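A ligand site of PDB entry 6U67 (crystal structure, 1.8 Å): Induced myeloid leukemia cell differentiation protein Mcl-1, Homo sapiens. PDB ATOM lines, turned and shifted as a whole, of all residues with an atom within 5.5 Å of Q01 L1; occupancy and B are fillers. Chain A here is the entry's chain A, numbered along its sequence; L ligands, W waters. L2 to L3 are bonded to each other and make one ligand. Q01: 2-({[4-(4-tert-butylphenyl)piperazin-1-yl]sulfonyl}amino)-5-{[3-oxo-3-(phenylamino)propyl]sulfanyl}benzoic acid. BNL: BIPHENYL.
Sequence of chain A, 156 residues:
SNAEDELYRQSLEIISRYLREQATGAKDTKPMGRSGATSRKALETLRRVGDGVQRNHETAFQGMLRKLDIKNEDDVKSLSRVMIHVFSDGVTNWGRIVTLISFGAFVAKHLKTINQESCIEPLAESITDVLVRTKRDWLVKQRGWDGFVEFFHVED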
ATOM      1  N   PHE A  61      27.353   8.202   2.904  1.00  0.00           N
ATOM      2  CA  PHE A  61      27.046   7.184   3.921  1.00  0.00           C
ATOM      3  C   PHE A  61      27.106   7.807   5.331  1.00  0.00           C
ATOM      4  O   PHE A  61      26.254   7.484   6.147  1.00  0.00           O
ATOM      5  CB  PHE A  61      28.001   5.972   3.794  1.00  0.00           C
ATOM      6  CG  PHE A  61      27.550   4.954   2.751  1.00  0.00           C
ATOM      7  CD1 PHE A  61      26.633   5.290   1.759  1.00  0.00           C
ATOM      8  CD2 PHE A  61      28.028   3.641   2.782  1.00  0.00           C
ATOM      9  CE1 PHE A  61      26.192   4.335   0.821  1.00  0.00           C
ATOM     10  CE2 PHE A  61      27.591   2.683   1.852  1.00  0.00           C
ATOM     11  CZ  PHE A  61      26.702   3.055   0.855  1.00  0.00           C
ATOM     12  N   MET A  64      23.946   9.972   5.821  1.00  0.00           N
ATOM     13  CA  MET A  64      22.768   9.121   6.042  1.00  0.00           C
ATOM     14  C   MET A  64      22.835   8.487   7.433  1.00  0.00           C
ATOM     15  O   MET A  64      21.831   8.494   8.132  1.00  0.00           O
ATOM     16  CB  MET A  64      22.678   8.009   4.969  1.00  0.00           C
ATOM     17  CG  MET A  64      22.159   8.547   3.658  1.00  0.00           C
ATOM     18  SD  MET A  64      21.809   7.223   2.475  1.00  0.00           S
ATOM     19  CE  MET A  64      23.409   6.802   2.038  1.00  0.00           C
ATOM     20  N   LEU A  68      19.945   9.292  10.361  1.00  0.00           N
ATOM     21  CA  LEU A  68      19.112   8.178  10.835  1.00  0.00           C
ATOM     22  C   LEU A  68      19.315   7.851  12.289  1.00  0.00           C
ATOM     23  O   LEU A  68      18.339   7.495  12.948  1.00  0.00           O
ATOM     24  CB  LEU A  68      19.350   6.914   9.980  1.00  0.00           C
ATOM     25  CG  LEU A  68      18.975   7.025   8.495  1.00  0.00           C
ATOM     26  CD1 LEU A  68      19.350   5.738   7.755  1.00  0.00           C
ATOM     27  CD2 LEU A  68      17.475   7.381   8.309  1.00  0.00           C
ATOM     28  N   ILE A  70      20.785   5.345  14.118  1.00  0.00           N
ATOM     29  CA  ILE A  70      20.329   4.016  14.470  1.00  0.00           C
ATOM     30  C   ILE A  70      21.174   3.561  15.651  1.00  0.00           C
ATOM     31  O   ILE A  70      22.400   3.489  15.520  1.00  0.00           O
ATOM     32  CB  ILE A  70      20.408   3.045  13.265  1.00  0.00           C
ATOM     33  CG1 ILE A  70      19.572   3.567  12.078  1.00  0.00           C
ATOM     34  CG2 ILE A  70      19.977   1.624  13.667  1.00  0.00           C
ATOM     35  CD1 ILE A  70      20.139   3.038  10.709  1.00  0.00           C
ATOM     36  N   VAL A  76      15.917   0.058  14.358  1.00  0.00           N
ATOM     37  CA  VAL A  76      16.013  -0.827  13.161  1.00  0.00           C
ATOM     38  C   VAL A  76      14.585  -1.212  12.681  1.00  0.00           C
ATOM     39  O   VAL A  76      14.311  -1.127  11.482  1.00  0.00           O
ATOM     40  CB  VAL A  76      16.888  -2.085  13.442  1.00  0.00           C
ATOM     41  CG1 VAL A  76      16.906  -3.037  12.234  1.00  0.00           C
ATOM     42  CG2 VAL A  76      18.313  -1.672  13.810  1.00  0.00           C
ATOM     43  N   LEU A  79      12.677   1.891  11.192  1.00  0.00           N
ATOM     44  CA  LEU A  79      13.260   2.219   9.905  1.00  0.00           C
ATOM     45  C   LEU A  79      12.921   1.156   8.835  1.00  0.00           C
ATOM     46  O   LEU A  79      12.662   1.516   7.690  1.00  0.00           O
ATOM     47  CB  LEU A  79      14.769   2.381  10.026  1.00  0.00           C
ATOM     48  CG  LEU A  79      15.490   3.151   8.900  1.00  0.00           C
ATOM     49  CD1 LEU A  79      14.728   4.383   8.475  1.00  0.00           C
ATOM     50  CD2 LEU A  79      16.844   3.555   9.348  1.00  0.00           C
ATOM     51  N   SER A  80      12.880  -0.140   9.194  1.00  0.00           N
ATOM     52  CA  SER A  80      12.583  -1.180   8.193  1.00  0.00           C
ATOM     53  C   SER A  80      11.178  -1.027   7.622  1.00  0.00           C
ATOM     54  O   SER A  80      11.014  -1.186   6.412  1.00  0.00           O
ATOM     55  CB  SER A  80      12.801  -2.568   8.774  1.00  0.00           C
ATOM     56  OG  SER A  80      11.897  -2.801   9.842  1.00  0.00           O
ATOM     57  N   MET A  83      11.481   1.855   5.127  1.00  0.00           N
ATOM     58  CA  MET A  83      12.396   1.531   4.033  1.00  0.00           C
ATOM     59  C   MET A  83      11.825   0.477   3.092  1.00  0.00           C
ATOM     60  O   MET A  83      12.212   0.466   1.930  1.00  0.00           O
ATOM     61  CB  MET A  83      13.789   1.144   4.526  1.00  0.00           C
ATOM     62  CG  MET A  83      14.495   2.356   5.165  1.00  0.00           C
ATOM     63  SD  MET A  83      14.641   3.700   3.947  1.00  0.00           S
ATOM     64  CE  MET A  83      15.662   4.946   4.932  1.00  0.00           C
ATOM     65  N   VAL A  86      10.157   2.904   0.789  1.00  0.00           N
ATOM     66  CA  VAL A  86      11.105   3.694  -0.016  1.00  0.00           C
ATOM     67  C   VAL A  86      11.823   2.808  -1.053  1.00  0.00           C
ATOM     68  O   VAL A  86      11.980   3.203  -2.216  1.00  0.00           O
ATOM     69  CB  VAL A  86      12.119   4.416   0.917  1.00  0.00           C
ATOM     70  CG1 VAL A  86      13.216   5.099   0.089  1.00  0.00           C
ATOM     71  CG2 VAL A  86      11.402   5.431   1.814  1.00  0.00           C
ATOM     72  N   PHE A  87      12.300   1.626  -0.625  1.00  0.00           N
ATOM     73  CA  PHE A  87      13.014   0.722  -1.529  1.00  0.00           C
ATOM     74  C   PHE A  87      12.107   0.174  -2.665  1.00  0.00           C
ATOM     75  O   PHE A  87      12.639  -0.304  -3.682  1.00  0.00           O
ATOM     76  CB  PHE A  87      13.666  -0.430  -0.742  1.00  0.00           C
ATOM     77  CG  PHE A  87      14.956  -0.912  -1.351  1.00  0.00           C
ATOM     78  CD1 PHE A  87      16.052  -0.053  -1.466  1.00  0.00           C
ATOM     79  CD2 PHE A  87      15.098  -2.215  -1.797  1.00  0.00           C
ATOM     80  CE1 PHE A  87      17.247  -0.492  -2.036  1.00  0.00           C
ATOM     81  CE2 PHE A  87      16.293  -2.653  -2.367  1.00  0.00           C
ATOM     82  CZ  PHE A  87      17.360  -1.789  -2.486  1.00  0.00           C
ATOM     83  N   ASP A  89      10.102   1.988  -4.567  1.00  0.00           N
ATOM     84  CA  ASP A  89       9.949   3.014  -5.585  1.00  0.00           C
ATOM     85  C   ASP A  89      11.191   3.134  -6.476  1.00  0.00           C
ATOM     86  O   ASP A  89      12.302   3.060  -5.998  1.00  0.00           O
ATOM     87  CB  ASP A  89       9.662   4.380  -4.935  1.00  0.00           C
ATOM     88  CG  ASP A  89       9.433   5.491  -5.934  1.00  0.00           C
ATOM     89  OD1 ASP A  89       8.414   5.449  -6.638  1.00  0.00           O
ATOM     90  OD2 ASP A  89      10.286   6.396  -6.013  1.00  0.00           O
ATOM     91  N   ARG A  96      21.845  -0.655  -7.045  1.00  0.00           N
ATOM     92  CA  ARG A  96      20.963  -0.253  -5.944  1.00  0.00           C
ATOM     93  C   ARG A  96      21.020  -1.288  -4.818  1.00  0.00           C
ATOM     94  O   ARG A  96      21.176  -0.920  -3.663  1.00  0.00           O
ATOM     95  CB  ARG A  96      19.501  -0.062  -6.426  1.00  0.00           C
ATOM     96  CG  ARG A  96      18.615   0.525  -5.317  1.00  0.00           C
ATOM     97  CD  ARG A  96      17.145   0.409  -5.683  1.00  0.00           C
ATOM     98  NE  ARG A  96      16.343   1.329  -4.878  1.00  0.00           N
ATOM     99  CZ  ARG A  96      15.047   1.593  -5.081  1.00  0.00           C
ATOM    100  NH1 ARG A  96      14.399   1.016  -6.084  1.00  0.00           N
ATOM    101  NH2 ARG A  96      14.400   2.434  -4.280  1.00  0.00           N
ATOM    102  N   THR A  99      24.299  -1.311  -2.928  1.00  0.00           N
ATOM    103  CA  THR A  99      24.438  -0.103  -2.100  1.00  0.00           C
ATOM    104  C   THR A  99      23.679  -0.313  -0.780  1.00  0.00           C
ATOM    105  O   THR A  99      24.174   0.076   0.277  1.00  0.00           O
ATOM    106  CB  THR A  99      23.973   1.139  -2.875  1.00  0.00           C
ATOM    107  OG1 THR A  99      24.732   1.209  -4.096  1.00  0.00           O
ATOM    108  CG2 THR A  99      24.167   2.433  -2.062  1.00  0.00           C
ATOM    109  N   LEU A 100      22.466  -0.907  -0.841  1.00  0.00           N
ATOM    110  CA  LEU A 100      21.705  -1.223   0.391  1.00  0.00           C
ATOM    111  C   LEU A 100      22.547  -2.109   1.341  1.00  0.00           C
ATOM    112  O   LEU A 100      22.651  -1.840   2.556  1.00  0.00           O
ATOM    113  CB  LEU A 100      20.408  -1.958   0.009  1.00  0.00           C
ATOM    114  CG  LEU A 100      19.610  -2.600   1.183  1.00  0.00           C
ATOM    115  CD1 LEU A 100      18.953  -1.516   2.054  1.00  0.00           C
ATOM    116  CD2 LEU A 100      18.554  -3.590   0.651  1.00  0.00           C
ATOM    117  N   ILE A 101      23.172  -3.150   0.792  1.00  0.00           N
ATOM    118  CA  ILE A 101      23.979  -4.086   1.622  1.00  0.00           C
ATOM    119  C   ILE A 101      25.206  -3.377   2.176  1.00  0.00           C
ATOM    120  O   ILE A 101      25.500  -3.502   3.372  1.00  0.00           O
ATOM    121  CB  ILE A 101      24.366  -5.355   0.818  1.00  0.00           C
ATOM    122  CG1 ILE A 101      23.083  -6.114   0.381  1.00  0.00           C
ATOM    123  CG2 ILE A 101      25.309  -6.263   1.632  1.00  0.00           C
ATOM    124  CD1 ILE A 101      23.334  -7.187  -0.674  1.00  0.00           C
ATOM    125  N   PHE A 103      25.536  -0.157   2.713  1.00  0.00           N
ATOM    126  CA  PHE A 103      25.098   0.771   3.772  1.00  0.00           C
ATOM    127  C   PHE A 103      24.832  -0.012   5.049  1.00  0.00           C
ATOM    128  O   PHE A 103      25.177   0.468   6.136  1.00  0.00           O
ATOM    129  CB  PHE A 103      23.866   1.599   3.351  1.00  0.00           C
ATOM    130  CG  PHE A 103      23.545   2.656   4.395  1.00  0.00           C
ATOM    131  CD1 PHE A 103      24.425   3.702   4.649  1.00  0.00           C
ATOM    132  CD2 PHE A 103      22.373   2.574   5.156  1.00  0.00           C
ATOM    133  CE1 PHE A 103      24.168   4.643   5.659  1.00  0.00           C
ATOM    134  CE2 PHE A 103      22.089   3.528   6.150  1.00  0.00           C
ATOM    135  CZ  PHE A 103      22.991   4.566   6.388  1.00  0.00           C
ATOM    136  N   LEU A 123      19.714  -6.083  12.331  1.00  0.00           N
ATOM    137  CA  LEU A 123      19.987  -5.201  11.198  1.00  0.00           C
ATOM    138  C   LEU A 123      20.091  -6.035   9.915  1.00  0.00           C
ATOM    139  O   LEU A 123      19.441  -5.689   8.929  1.00  0.00           O
ATOM    140  CB  LEU A 123      21.288  -4.405  11.413  1.00  0.00           C
ATOM    141  CG  LEU A 123      21.823  -3.597  10.221  1.00  0.00           C
ATOM    142  CD1 LEU A 123      20.869  -2.480   9.827  1.00  0.00           C
ATOM    143  CD2 LEU A 123      23.184  -3.052  10.530  1.00  0.00           C
ATOM    144  N   SER A 126      16.596  -7.191   8.875  1.00  0.00           N
ATOM    145  CA  SER A 126      15.813  -6.105   8.297  1.00  0.00           C
ATOM    146  C   SER A 126      16.313  -5.762   6.895  1.00  0.00           C
ATOM    147  O   SER A 126      15.492  -5.515   6.007  1.00  0.00           O
ATOM    148  CB  SER A 126      15.828  -4.883   9.198  1.00  0.00           C
ATOM    149  OG  SER A 126      15.171  -5.203  10.412  1.00  0.00           O
ATOM    150  N   ILE A 127      17.638  -5.744   6.684  1.00  0.00           N
ATOM    151  CA  ILE A 127      18.189  -5.490   5.340  1.00  0.00           C
ATOM    152  C   ILE A 127      17.652  -6.597   4.406  1.00  0.00           C
ATOM    153  O   ILE A 127      17.224  -6.315   3.280  1.00  0.00           O
ATOM    154  CB  ILE A 127      19.750  -5.452   5.333  1.00  0.00           C
ATOM    155  CG1 ILE A 127      20.329  -4.206   6.091  1.00  0.00           C
ATOM    156  CG2 ILE A 127      20.308  -5.552   3.879  1.00  0.00           C
ATOM    157  CD1 ILE A 127      20.455  -2.808   5.268  1.00  0.00           C
ATOM    158  N   VAL A 130      13.842  -6.069   3.716  1.00  0.00           N
ATOM    159  CA  VAL A 130      13.662  -4.977   2.777  1.00  0.00           C
ATOM    160  C   VAL A 130      13.942  -5.472   1.357  1.00  0.00           C
ATOM    161  O   VAL A 130      13.116  -5.300   0.471  1.00  0.00           O
ATOM    162  CB  VAL A 130      14.539  -3.750   3.150  1.00  0.00           C
ATOM    163  CG1 VAL A 130      14.685  -2.781   1.982  1.00  0.00           C
ATOM    164  CG2 VAL A 130      13.986  -3.046   4.388  1.00  0.00           C
HETATM  165  C1  Q01 L   1      13.012  10.675   1.040  1.00  0.00           C
HETATM  166  C2  Q01 L   1      13.279  11.789   1.814  1.00  0.00           C
HETATM  167  C3  Q01 L   1      12.269  12.379   2.556  1.00  0.00           C
HETATM  168  C4  Q01 L   1      10.987  11.859   2.518  1.00  0.00           C
HETATM  169  C5  Q01 L   1      10.712  10.775   1.710  1.00  0.00           C
HETATM  170  C6  Q01 L   1      11.714  10.180   0.971  1.00  0.00           C
HETATM  171  C8  Q01 L   1      16.307   9.318  -1.678  1.00  0.00           C
HETATM  172  C11 Q01 L   1      17.968   5.043  -1.956  1.00  0.00           C
HETATM  173  C12 Q01 L   1      17.053   3.922  -2.390  1.00  0.00           C
HETATM  174  C13 Q01 L   1      19.233   4.808  -1.362  1.00  0.00           C
HETATM  175  C14 Q01 L   1      18.539   2.355   1.106  1.00  0.00           C
HETATM  176  C15 Q01 L   1      17.615   3.066   2.062  1.00  0.00           C
HETATM  177  C16 Q01 L   1      18.181   2.177   4.384  1.00  0.00           C
HETATM  178  C21 Q01 L   1      17.864  -1.964   7.544  1.00  0.00           C
HETATM  179  C23 Q01 L   1      15.851  -0.594   7.849  1.00  0.00           C
HETATM  180  C24 Q01 L   1      17.206   0.139   5.244  1.00  0.00           C
HETATM  181  C25 Q01 L   1      17.421   1.013   4.195  1.00  0.00           C
HETATM  182  C26 Q01 L   1      19.442   4.029   3.258  1.00  0.00           C
HETATM  183  C27 Q01 L   1      20.451   3.353   2.372  1.00  0.00           C
HETATM  184  O4  Q01 L   1      21.832   3.829  -0.084  1.00  0.00           O
HETATM  185  S1  Q01 L   1      20.710   2.979  -0.272  1.00  0.00           S
HETATM  186  O3  Q01 L   1      20.897   1.601  -0.601  1.00  0.00           O
HETATM  187  N2  Q01 L   1      19.854   3.032   1.057  1.00  0.00           N
HETATM  188  N3  Q01 L   1      18.252   3.185   3.377  1.00  0.00           N
HETATM  189  C19 Q01 L   1      17.751   0.356   6.504  1.00  0.00           C
HETATM  190  C20 Q01 L   1      17.373  -0.526   7.704  1.00  0.00           C
HETATM  191  C22 Q01 L   1      17.939   0.007   9.030  1.00  0.00           C
HETATM  192  C18 Q01 L   1      18.562   1.478   6.669  1.00  0.00           C
HETATM  193  C17 Q01 L   1      18.769   2.378   5.635  1.00  0.00           C
HETATM  194  N1  Q01 L   1      19.834   3.528  -1.486  1.00  0.00           N
HETATM  195  O2  Q01 L   1      15.841   4.081  -2.509  1.00  0.00           O
HETATM  196  O1  Q01 L   1      17.622   2.796  -2.697  1.00  0.00           O
HETATM  197  C10 Q01 L   1      17.549   6.367  -2.120  1.00  0.00           C
HETATM  198  C28 Q01 L   1      19.955   5.869  -0.827  1.00  0.00           C
HETATM  199  C29 Q01 L   1      19.515   7.171  -0.985  1.00  0.00           C
HETATM  200  C9  Q01 L   1      18.351   7.428  -1.685  1.00  0.00           C
HETATM  201  S   Q01 L   1      18.011   9.090  -2.186  1.00  0.00           S
HETATM  202  C7  Q01 L   1      16.129   8.995  -0.214  1.00  0.00           C
HETATM  203  C   Q01 L   1      15.342  10.141   0.353  1.00  0.00           C
HETATM  204  O   Q01 L   1      15.881  11.189   0.703  1.00  0.00           O
HETATM  205  N   Q01 L   1      14.021   9.912   0.409  1.00  0.00           N
HETATM  206  C11 Q01 L   2      18.331   7.684  -8.312  1.00  0.00           C
HETATM  207  C12 Q01 L   2      17.038   7.298  -8.966  1.00  0.00           C
HETATM  208  C13 Q01 L   2      19.479   6.853  -8.373  1.00  0.00           C
HETATM  209  O4  Q01 L   2      21.758   4.798  -9.587  1.00  0.00           O
HETATM  210  S1  Q01 L   2      20.495   4.405  -9.044  1.00  0.00           S
HETATM  211  O3  Q01 L   2      19.859   3.235  -9.551  1.00  0.00           O
HETATM  212  N1  Q01 L   2      19.451   5.653  -9.133  1.00  0.00           N
HETATM  213  O2  Q01 L   2      16.081   8.144  -8.786  1.00  0.00           O
HETATM  214  O1  Q01 L   2      16.892   6.273  -9.598  1.00  0.00           O
HETATM  215  C10 Q01 L   2      18.400   8.879  -7.605  1.00  0.00           C
HETATM  216  C28 Q01 L   2      20.644   7.245  -7.696  1.00  0.00           C
HETATM  217  C29 Q01 L   2      20.669   8.426  -6.967  1.00  0.00           C
HETATM  218  C9  Q01 L   2      19.562   9.249  -6.935  1.00  0.00           C
HETATM  219  S   Q01 L   2      19.576  10.801  -6.086  1.00  0.00           S
HETATM  220  C1  BNL L   3      20.224   3.928  -4.738  1.00  0.00           C
HETATM  221  C2  BNL L   3      19.771   4.024  -6.055  1.00  0.00           C
HETATM  222  C3  BNL L   3      20.716   3.724  -7.047  1.00  0.00           C
HETATM  223  C4  BNL L   3      22.066   3.438  -6.776  1.00  0.00           C
HETATM  224  C5  BNL L   3      22.477   3.389  -5.440  1.00  0.00           C
HETATM  225  C6  BNL L   3      21.550   3.642  -4.439  1.00  0.00           C
HETATM  226  C12 BNL L   3      16.187   3.803  -7.378  1.00  0.00           C
HETATM  227  C13 BNL L   3      15.555   4.819  -6.622  1.00  0.00           C
HETATM  228  C14 BNL L   3      16.303   5.595  -5.722  1.00  0.00           C
HETATM  229  C15 BNL L   3      17.672   5.329  -5.580  1.00  0.00           C
HETATM  230  C16 BNL L   3      18.317   4.331  -6.338  1.00  0.00           C
HETATM  231  C17 BNL L   3      17.567   3.566  -7.257  1.00  0.00           C
HETATM  232  C14 Q01 L   4      25.285   6.165  -6.125  1.00  0.00           C
HETATM  233  C15 Q01 L   4      25.213   4.861  -6.895  1.00  0.00           C
HETATM  234  C16 Q01 L   4      26.615   2.874  -7.321  1.00  0.00           C
HETATM  235  C21 Q01 L   4      26.947  -1.683  -9.474  1.00  0.00           C
HETATM  236  C23 Q01 L   4      29.040  -0.656 -10.305  1.00  0.00           C
HETATM  237  C24 Q01 L   4      27.333   0.582  -7.681  1.00  0.00           C
HETATM  238  C25 Q01 L   4      26.946   1.609  -6.830  1.00  0.00           C
HETATM  239  C26 Q01 L   4      26.110   3.648  -5.031  1.00  0.00           C
HETATM  240  C27 Q01 L   4      26.188   4.904  -4.196  1.00  0.00           C
HETATM  241  O4  Q01 L   4      24.637   8.207  -4.060  1.00  0.00           O
HETATM  242  S1  Q01 L   4      24.325   6.850  -3.725  1.00  0.00           S
HETATM  243  O3  Q01 L   4      24.395   6.448  -2.362  1.00  0.00           O
HETATM  244  N2  Q01 L   4      25.215   5.906  -4.670  1.00  0.00           N
HETATM  245  N3  Q01 L   4      26.260   3.933  -6.466  1.00  0.00           N
HETATM  246  C19 Q01 L   4      27.358   0.761  -9.062  1.00  0.00           C
HETATM  247  C20 Q01 L   4      27.556  -0.414 -10.033  1.00  0.00           C
HETATM  248  C22 Q01 L   4      26.853  -0.180 -11.374  1.00  0.00           C
HETATM  249  C18 Q01 L   4      27.048   2.032  -9.553  1.00  0.00           C
HETATM  250  C17 Q01 L   4      26.672   3.055  -8.710  1.00  0.00           C
HETATM  251  O   HOH W   1      13.416   5.277  -3.298  1.00  0.00           O
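The guanidinium group (NH2) of Arg 96 is in salt-bridge range of an oxygen (O2) of Q01 L1 (2.8 Å).
The backbone NH (N) of Leu 100 is in hydrogen-bond range of an oxygen (O3) of Q01 L1 (3.0 Å).
The guanidinium group of Arg 96 sits at hydrogen-bond distance from the backbone carbonyl oxygen of Phe 87, 3.3 Å away.
The backbone carbonyl oxygen of Val 86 sits at hydrogen-bond distance from the guanidinium group of Arg 96, 3.3 Å away.
NH2 of Arg 96 lies within hydrogen-bond range of O of Asp 89 (2.8 Å).
OG of Ser 80 sits at hydrogen-bond distance from O of Val 76.
A nitrogen (N3) of Q01 L1 lies close to the side-chain sulfur (SD) of Met 83, 3.7 Å away.
Residues that only touch Q01 L1: Ser 80 (3.3 Å), Thr 99 (3.4 Å), Phe 87 (3.4 Å), Phe 103 (3.5 Å), Ile 127 (3.6 Å), Leu 79 (3.6 Å), Leu 123 (3.8 Å), Val 86 (3.8 Å), Ser 126 (3.9 Å), Met 64 (3.98 Å) and Val 76 (3.98 Å).
Hydrophobic or aromatic side chains within 4 Å of Q01 L1: Met 64, Leu 79, Met 83, Val 86, Phe 87, Leu 100, Phe 103, Leu 123 and Ile 127.
The nearest printed residue that does not touch Q01 L1 is Leu 68 (4.02 Å).
Water W1 lies within hydrogen-bond range of the backbone carbonyl oxygen of Val 86 (2.7 Å), an oxygen (O2) of Q01 L1 (2.8 Å) and the guanidinium group of Arg 96 (3.2 Å).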
